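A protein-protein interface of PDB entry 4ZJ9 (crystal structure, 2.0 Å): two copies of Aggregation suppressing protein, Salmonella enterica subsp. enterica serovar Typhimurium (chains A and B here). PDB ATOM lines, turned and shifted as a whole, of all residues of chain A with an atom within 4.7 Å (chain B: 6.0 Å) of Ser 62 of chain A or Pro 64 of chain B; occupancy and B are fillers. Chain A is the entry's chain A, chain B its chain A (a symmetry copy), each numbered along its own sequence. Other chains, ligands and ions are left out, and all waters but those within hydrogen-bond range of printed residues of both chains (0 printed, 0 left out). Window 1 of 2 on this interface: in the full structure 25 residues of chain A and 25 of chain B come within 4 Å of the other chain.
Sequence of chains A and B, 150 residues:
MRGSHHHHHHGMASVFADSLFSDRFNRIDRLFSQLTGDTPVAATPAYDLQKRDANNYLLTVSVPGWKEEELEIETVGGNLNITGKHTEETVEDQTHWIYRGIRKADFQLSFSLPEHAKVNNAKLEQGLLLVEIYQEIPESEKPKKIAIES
Ser 62 of chain A touches Pro 64 of chain B, and with the chains exchanged Pro 64 of chain A touches Ser 62 of chain B.
Pro 64 of chain A touches Gly 127 of chain B, and with the chains exchanged Gly 127 of chain A touches Pro 64 of chain B.
Gly 127 of chain A touches its own counterpart, Gly 127 of chain B.
5 positions are printed for both chains.
Of the 12 pairs that touch across the chains among the printed residues, 5 have their exchanged pair printed and touching as well.
Of the printed residues of chain B, Ser 62 of chain A touches Pro 64 and Ile 102.
Printed residues of chain A within 4 Å of Pro 64 of chain B: Ser 62, Gln 126 and Gly 127.
Printed residues of chain B within 4 Å of Gly 127 of chain A: Pro 64 (3.8 Å) and Gly 127 (3.4 Å).
Printed residues of chain A within 4 Å of Trp 66 of chain B: Gln 126 (3.0 Å).
The nearest printed residue of chain B that does not touch Gly 127 of chain A is Gly 65 of chain B (5.0 Å).
NE2 of Gln 126 of chain A lies within hydrogen-bond range of O of Trp 66 of chain B (3.0 Å).
N of Gly 127 of chain B sits close to N of Gly 127 of chain A, 3.4 Å away.
The backbone carbonyl oxygen (O) of Gln 126 of chain A sits at hydrogen-bond distance from the backbone NH (N) of Gly 65 of chain B (2.8 Å).
Among the printed residues, merely in contact across the chains: Pro 64 of chain A with Ser 62 of chain B (3.4 Å), Ser 62 of chain A with Pro 64 of chain B (3.4 Å), Gln 126 of chain A with Pro 64 of chain B (3.5 Å), Gln 126 of chain A with Gly 127 of chain B (3.6 Å), Leu 128 of chain A with Gly 65 of chain B (3.6 Å), Thr 60 of chain A with Ile 102 of chain B (3.7 Å), Pro 64 of chain A with Gly 127 of chain B (3.8 Å), Gly 127 of chain A with Pro 64 of chain B (3.8 Å) and Ser 62 of chain A with Ile 102 of chain B (3.99 Å).
N of Val 63 of chain A sits at hydrogen-bond distance from O of Gly 127 of chain A (2.7 Å).
The backbone NH (N) of Ser 62 of chain A sits at hydrogen-bond distance from the backbone carbonyl oxygen (O) of Ala 46 of chain A, 3.0 Å away.
The backbone carbonyl oxygen (O) of Gly 127 of chain B is in hydrogen-bond range of the backbone NH (N) of Val 63 of chain B (2.7 Å).
The side-chain amino group of Lys 104 of chain B sits at hydrogen-bond distance from the backbone carbonyl oxygen of Gly 65 of chain B (3.0 Å).
Hydrophobic or aromatic side chains of chain B within 4 Å of the printed part of chain A: Pro 64 and Ile 102.
Among the printed residues, 12 pairs touch across the chains.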
ATOM      1  N   PRO A  45     -26.903  -2.759  13.936  1.00  0.00           N
ATOM      2  CA  PRO A  45     -26.646  -1.386  13.564  1.00  0.00           C
ATOM      3  C   PRO A  45     -27.571  -0.866  12.534  1.00  0.00           C
ATOM      4  O   PRO A  45     -27.928  -1.564  11.555  1.00  0.00           O
ATOM      5  CB  PRO A  45     -25.197  -1.427  13.033  1.00  0.00           C
ATOM      6  CG  PRO A  45     -24.621  -2.684  13.527  1.00  0.00           C
ATOM      7  CD  PRO A  45     -25.778  -3.642  13.571  1.00  0.00           C
ATOM      8  N   ALA A  46     -27.954   0.396  12.696  1.00  0.00           N
ATOM      9  CA  ALA A  46     -28.684   1.083  11.668  1.00  0.00           C
ATOM     10  C   ALA A  46     -27.856   1.134  10.392  1.00  0.00           C
ATOM     11  O   ALA A  46     -26.635   1.183  10.447  1.00  0.00           O
ATOM     12  CB  ALA A  46     -29.020   2.500  12.171  1.00  0.00           C
ATOM     13  N   THR A  60     -24.132   2.155   3.945  1.00  0.00           N
ATOM     14  CA  THR A  60     -23.567   2.849   5.101  1.00  0.00           C
ATOM     15  C   THR A  60     -24.051   2.212   6.378  1.00  0.00           C
ATOM     16  O   THR A  60     -25.265   2.157   6.647  1.00  0.00           O
ATOM     17  CB  THR A  60     -24.013   4.365   5.054  1.00  0.00           C
ATOM     18  OG1 THR A  60     -23.483   4.926   3.855  1.00  0.00           O
ATOM     19  CG2 THR A  60     -23.469   5.142   6.209  1.00  0.00           C
ATOM     20  N   VAL A  61     -23.107   1.750   7.197  1.00  0.00           N
ATOM     21  CA  VAL A  61     -23.469   1.147   8.456  1.00  0.00           C
ATOM     22  C   VAL A  61     -22.991   2.045   9.606  1.00  0.00           C
ATOM     23  O   VAL A  61     -21.851   2.488   9.623  1.00  0.00           O
ATOM     24  CB  VAL A  61     -22.833  -0.242   8.591  1.00  0.00           C
ATOM     25  CG1 VAL A  61     -23.369  -0.971   9.826  1.00  0.00           C
ATOM     26  CG2 VAL A  61     -23.142  -1.050   7.358  1.00  0.00           C
ATOM     27  N   SER A  62     -23.900   2.288  10.557  1.00  0.00           N
ATOM     28  CA  SER A  62     -23.604   3.123  11.752  1.00  0.00           C
ATOM     29  C   SER A  62     -22.845   2.251  12.770  1.00  0.00           C
ATOM     30  O   SER A  62     -23.417   1.304  13.296  1.00  0.00           O
ATOM     31  CB  SER A  62     -24.860   3.658  12.421  1.00  0.00           C
ATOM     32  OG  SER A  62     -24.494   4.547  13.524  1.00  0.00           O
ATOM     33  N   VAL A  63     -21.558   2.537  12.979  1.00  0.00           N
ATOM     34  CA  VAL A  63     -20.730   1.717  13.830  1.00  0.00           C
ATOM     35  C   VAL A  63     -19.855   2.629  14.740  1.00  0.00           C
ATOM     36  O   VAL A  63     -18.620   2.558  14.702  1.00  0.00           O
ATOM     37  CB  VAL A  63     -19.863   0.719  13.045  1.00  0.00           C
ATOM     38  CG1 VAL A  63     -20.730  -0.448  12.542  1.00  0.00           C
ATOM     39  CG2 VAL A  63     -19.128   1.427  11.966  1.00  0.00           C
ATOM     40  N   PRO A  64     -20.506   3.465  15.595  1.00  0.00           N
ATOM     41  CA  PRO A  64     -19.682   4.413  16.372  1.00  0.00           C
ATOM     42  C   PRO A  64     -18.902   3.635  17.419  1.00  0.00           C
ATOM     43  O   PRO A  64     -19.421   2.634  17.954  1.00  0.00           O
ATOM     44  CB  PRO A  64     -20.718   5.335  16.974  1.00  0.00           C
ATOM     45  CG  PRO A  64     -22.005   4.546  17.022  1.00  0.00           C
ATOM     46  CD  PRO A  64     -21.933   3.712  15.772  1.00  0.00           C
ATOM     47  N   GLN A 126     -15.685   8.513  10.692  1.00  0.00           N
ATOM     48  CA  GLN A 126     -16.747   9.139  11.499  1.00  0.00           C
ATOM     49  C   GLN A 126     -17.789   8.288  12.049  1.00  0.00           C
ATOM     50  O   GLN A 126     -18.932   8.709  12.172  1.00  0.00           O
ATOM     51  CB  GLN A 126     -17.335  10.279  10.681  1.00  0.00           C
ATOM     52  CG  GLN A 126     -16.151  11.208  10.361  1.00  0.00           C
ATOM     53  CD  GLN A 126     -16.536  12.645  10.430  1.00  0.00           C
ATOM     54  OE1 GLN A 126     -17.060  13.187   9.449  1.00  0.00           O
ATOM     55  NE2 GLN A 126     -16.338  13.269  11.593  1.00  0.00           N
ATOM     56  N   GLY A 127     -17.397   7.105  12.495  1.00  0.00           N
ATOM     57  CA  GLY A 127     -18.313   6.145  13.107  1.00  0.00           C
ATOM     58  C   GLY A 127     -19.243   5.479  12.109  1.00  0.00           C
ATOM     59  O   GLY A 127     -20.224   4.852  12.493  1.00  0.00           O
ATOM     60  N   LEU A 128     -18.886   5.565  10.827  1.00  0.00           N
ATOM     61  CA  LEU A 128     -19.651   5.035   9.750  1.00  0.00           C
ATOM     62  C   LEU A 128     -18.795   4.081   8.917  1.00  0.00           C
ATOM     63  O   LEU A 128     -17.613   4.322   8.714  1.00  0.00           O
ATOM     64  CB  LEU A 128     -20.252   6.130   8.813  1.00  0.00           C
ATOM     65  CG  LEU A 128     -21.187   7.129   9.496  1.00  0.00           C
ATOM     66  CD1 LEU A 128     -21.598   8.203   8.498  1.00  0.00           C
ATOM     67  CD2 LEU A 128     -22.346   6.458  10.177  1.00  0.00           C
ATOM     68  N   SER B  62     -22.381   9.647  21.554  1.00  0.00           N
ATOM     69  CA  SER B  62     -22.441   8.883  20.279  1.00  0.00           C
ATOM     70  C   SER B  62     -22.942   9.831  19.174  1.00  0.00           C
ATOM     71  O   SER B  62     -24.085  10.268  19.227  1.00  0.00           O
ATOM     72  CB  SER B  62     -23.385   7.693  20.353  1.00  0.00           C
ATOM     73  OG  SER B  62     -23.320   6.931  19.105  1.00  0.00           O
ATOM     74  N   VAL B  63     -22.064  10.190  18.235  1.00  0.00           N
ATOM     75  CA  VAL B  63     -22.398  11.157  17.217  1.00  0.00           C
ATOM     76  C   VAL B  63     -21.878  10.661  15.836  1.00  0.00           C
ATOM     77  O   VAL B  63     -21.072  11.339  15.186  1.00  0.00           O
ATOM     78  CB  VAL B  63     -21.877  12.569  17.534  1.00  0.00           C
ATOM     79  CG1 VAL B  63     -22.749  13.218  18.623  1.00  0.00           C
ATOM     80  CG2 VAL B  63     -20.433  12.509  17.877  1.00  0.00           C
ATOM     81  N   PRO B  64     -22.375   9.483  15.369  1.00  0.00           N
ATOM     82  CA  PRO B  64     -21.795   8.953  14.118  1.00  0.00           C
ATOM     83  C   PRO B  64     -22.251   9.828  12.962  1.00  0.00           C
ATOM     84  O   PRO B  64     -23.391  10.334  12.987  1.00  0.00           O
ATOM     85  CB  PRO B  64     -22.363   7.553  14.057  1.00  0.00           C
ATOM     86  CG  PRO B  64     -23.634   7.581  14.873  1.00  0.00           C
ATOM     87  CD  PRO B  64     -23.297   8.536  15.985  1.00  0.00           C
ATOM     88  N   GLY B  65     -21.363  10.050  11.995  1.00  0.00           N
ATOM     89  CA  GLY B  65     -21.664  10.926  10.871  1.00  0.00           C
ATOM     90  C   GLY B  65     -21.632  12.425  11.092  1.00  0.00           C
ATOM     91  O   GLY B  65     -21.822  13.231  10.153  1.00  0.00           O
ATOM     92  N   TRP B  66     -21.466  12.830  12.335  1.00  0.00           N
ATOM     93  CA  TRP B  66     -21.376  14.280  12.654  1.00  0.00           C
ATOM     94  C   TRP B  66     -19.986  14.806  12.347  1.00  0.00           C
ATOM     95  O   TRP B  66     -18.991  14.099  12.633  1.00  0.00           O
ATOM     96  CB  TRP B  66     -21.738  14.530  14.127  1.00  0.00           C
ATOM     97  CG  TRP B  66     -23.179  14.386  14.395  1.00  0.00           C
ATOM     98  CD1 TRP B  66     -23.862  13.248  14.617  1.00  0.00           C
ATOM     99  CD2 TRP B  66     -24.117  15.451  14.455  1.00  0.00           C
ATOM    100  NE1 TRP B  66     -25.167  13.515  14.821  1.00  0.00           N
ATOM    101  CE2 TRP B  66     -25.357  14.882  14.742  1.00  0.00           C
ATOM    102  CE3 TRP B  66     -24.016  16.823  14.264  1.00  0.00           C
ATOM    103  CZ2 TRP B  66     -26.502  15.621  14.852  1.00  0.00           C
ATOM    104  CZ3 TRP B  66     -25.171  17.581  14.373  1.00  0.00           C
ATOM    105  CH2 TRP B  66     -26.407  16.972  14.681  1.00  0.00           C
ATOM    106  N   ILE B 102     -30.538   5.366   9.069  1.00  0.00           N
ATOM    107  CA  ILE B 102     -29.701   6.216   9.910  1.00  0.00           C
ATOM    108  C   ILE B 102     -30.329   7.612   9.959  1.00  0.00           C
ATOM    109  O   ILE B 102     -30.408   8.313   8.938  1.00  0.00           O
ATOM    110  CB  ILE B 102     -28.291   6.349   9.333  1.00  0.00           C
ATOM    111  CG1 ILE B 102     -27.552   5.031   9.421  1.00  0.00           C
ATOM    112  CG2 ILE B 102     -27.469   7.346  10.144  1.00  0.00           C
ATOM    113  CD1 ILE B 102     -26.167   5.050   8.782  1.00  0.00           C
ATOM    114  N   LYS B 104     -30.403  11.459  11.575  1.00  0.00           N
ATOM    115  CA  LYS B 104     -29.499  12.456  12.127  1.00  0.00           C
ATOM    116  C   LYS B 104     -30.369  13.721  12.404  1.00  0.00           C
ATOM    117  O   LYS B 104     -31.005  14.283  11.509  1.00  0.00           O
ATOM    118  CB  LYS B 104     -28.342  12.705  11.149  1.00  0.00           C
ATOM    119  CG  LYS B 104     -27.151  13.494  11.712  1.00  0.00           C
ATOM    120  CD  LYS B 104     -26.093  13.773  10.633  1.00  0.00           C
ATOM    121  CE  LYS B 104     -25.383  15.108  10.815  1.00  0.00           C
ATOM    122  NZ  LYS B 104     -24.140  15.115   9.977  1.00  0.00           N
ATOM    123  N   GLY B 127     -16.771   8.438  15.528  1.00  0.00           N
ATOM    124  CA  GLY B 127     -18.197   8.701  15.706  1.00  0.00           C
ATOM    125  C   GLY B 127     -18.583   8.974  17.149  1.00  0.00           C
ATOM    126  O   GLY B 127     -19.760   8.958  17.493  1.00  0.00           O
ATOM    127  N   LEU B 128     -17.584   9.292  17.973  1.00  0.00           N
ATOM    128  CA  LEU B 128     -17.750   9.545  19.364  1.00  0.00           C
ATOM    129  C   LEU B 128     -17.187  10.922  19.719  1.00  0.00           C
ATOM    130  O   LEU B 128     -16.170  11.336  19.179  1.00  0.00           O
ATOM    131  CB  LEU B 128     -17.080   8.471  20.277  1.00  0.00           C
ATOM    132  CG  LEU B 128     -17.588   7.041  20.082  1.00  0.00           C
ATOM    133  CD1 LEU B 128     -16.769   6.090  20.942  1.00  0.00           C
ATOM    134  CD2 LEU B 128     -19.071   6.926  20.292  1.00  0.00           C
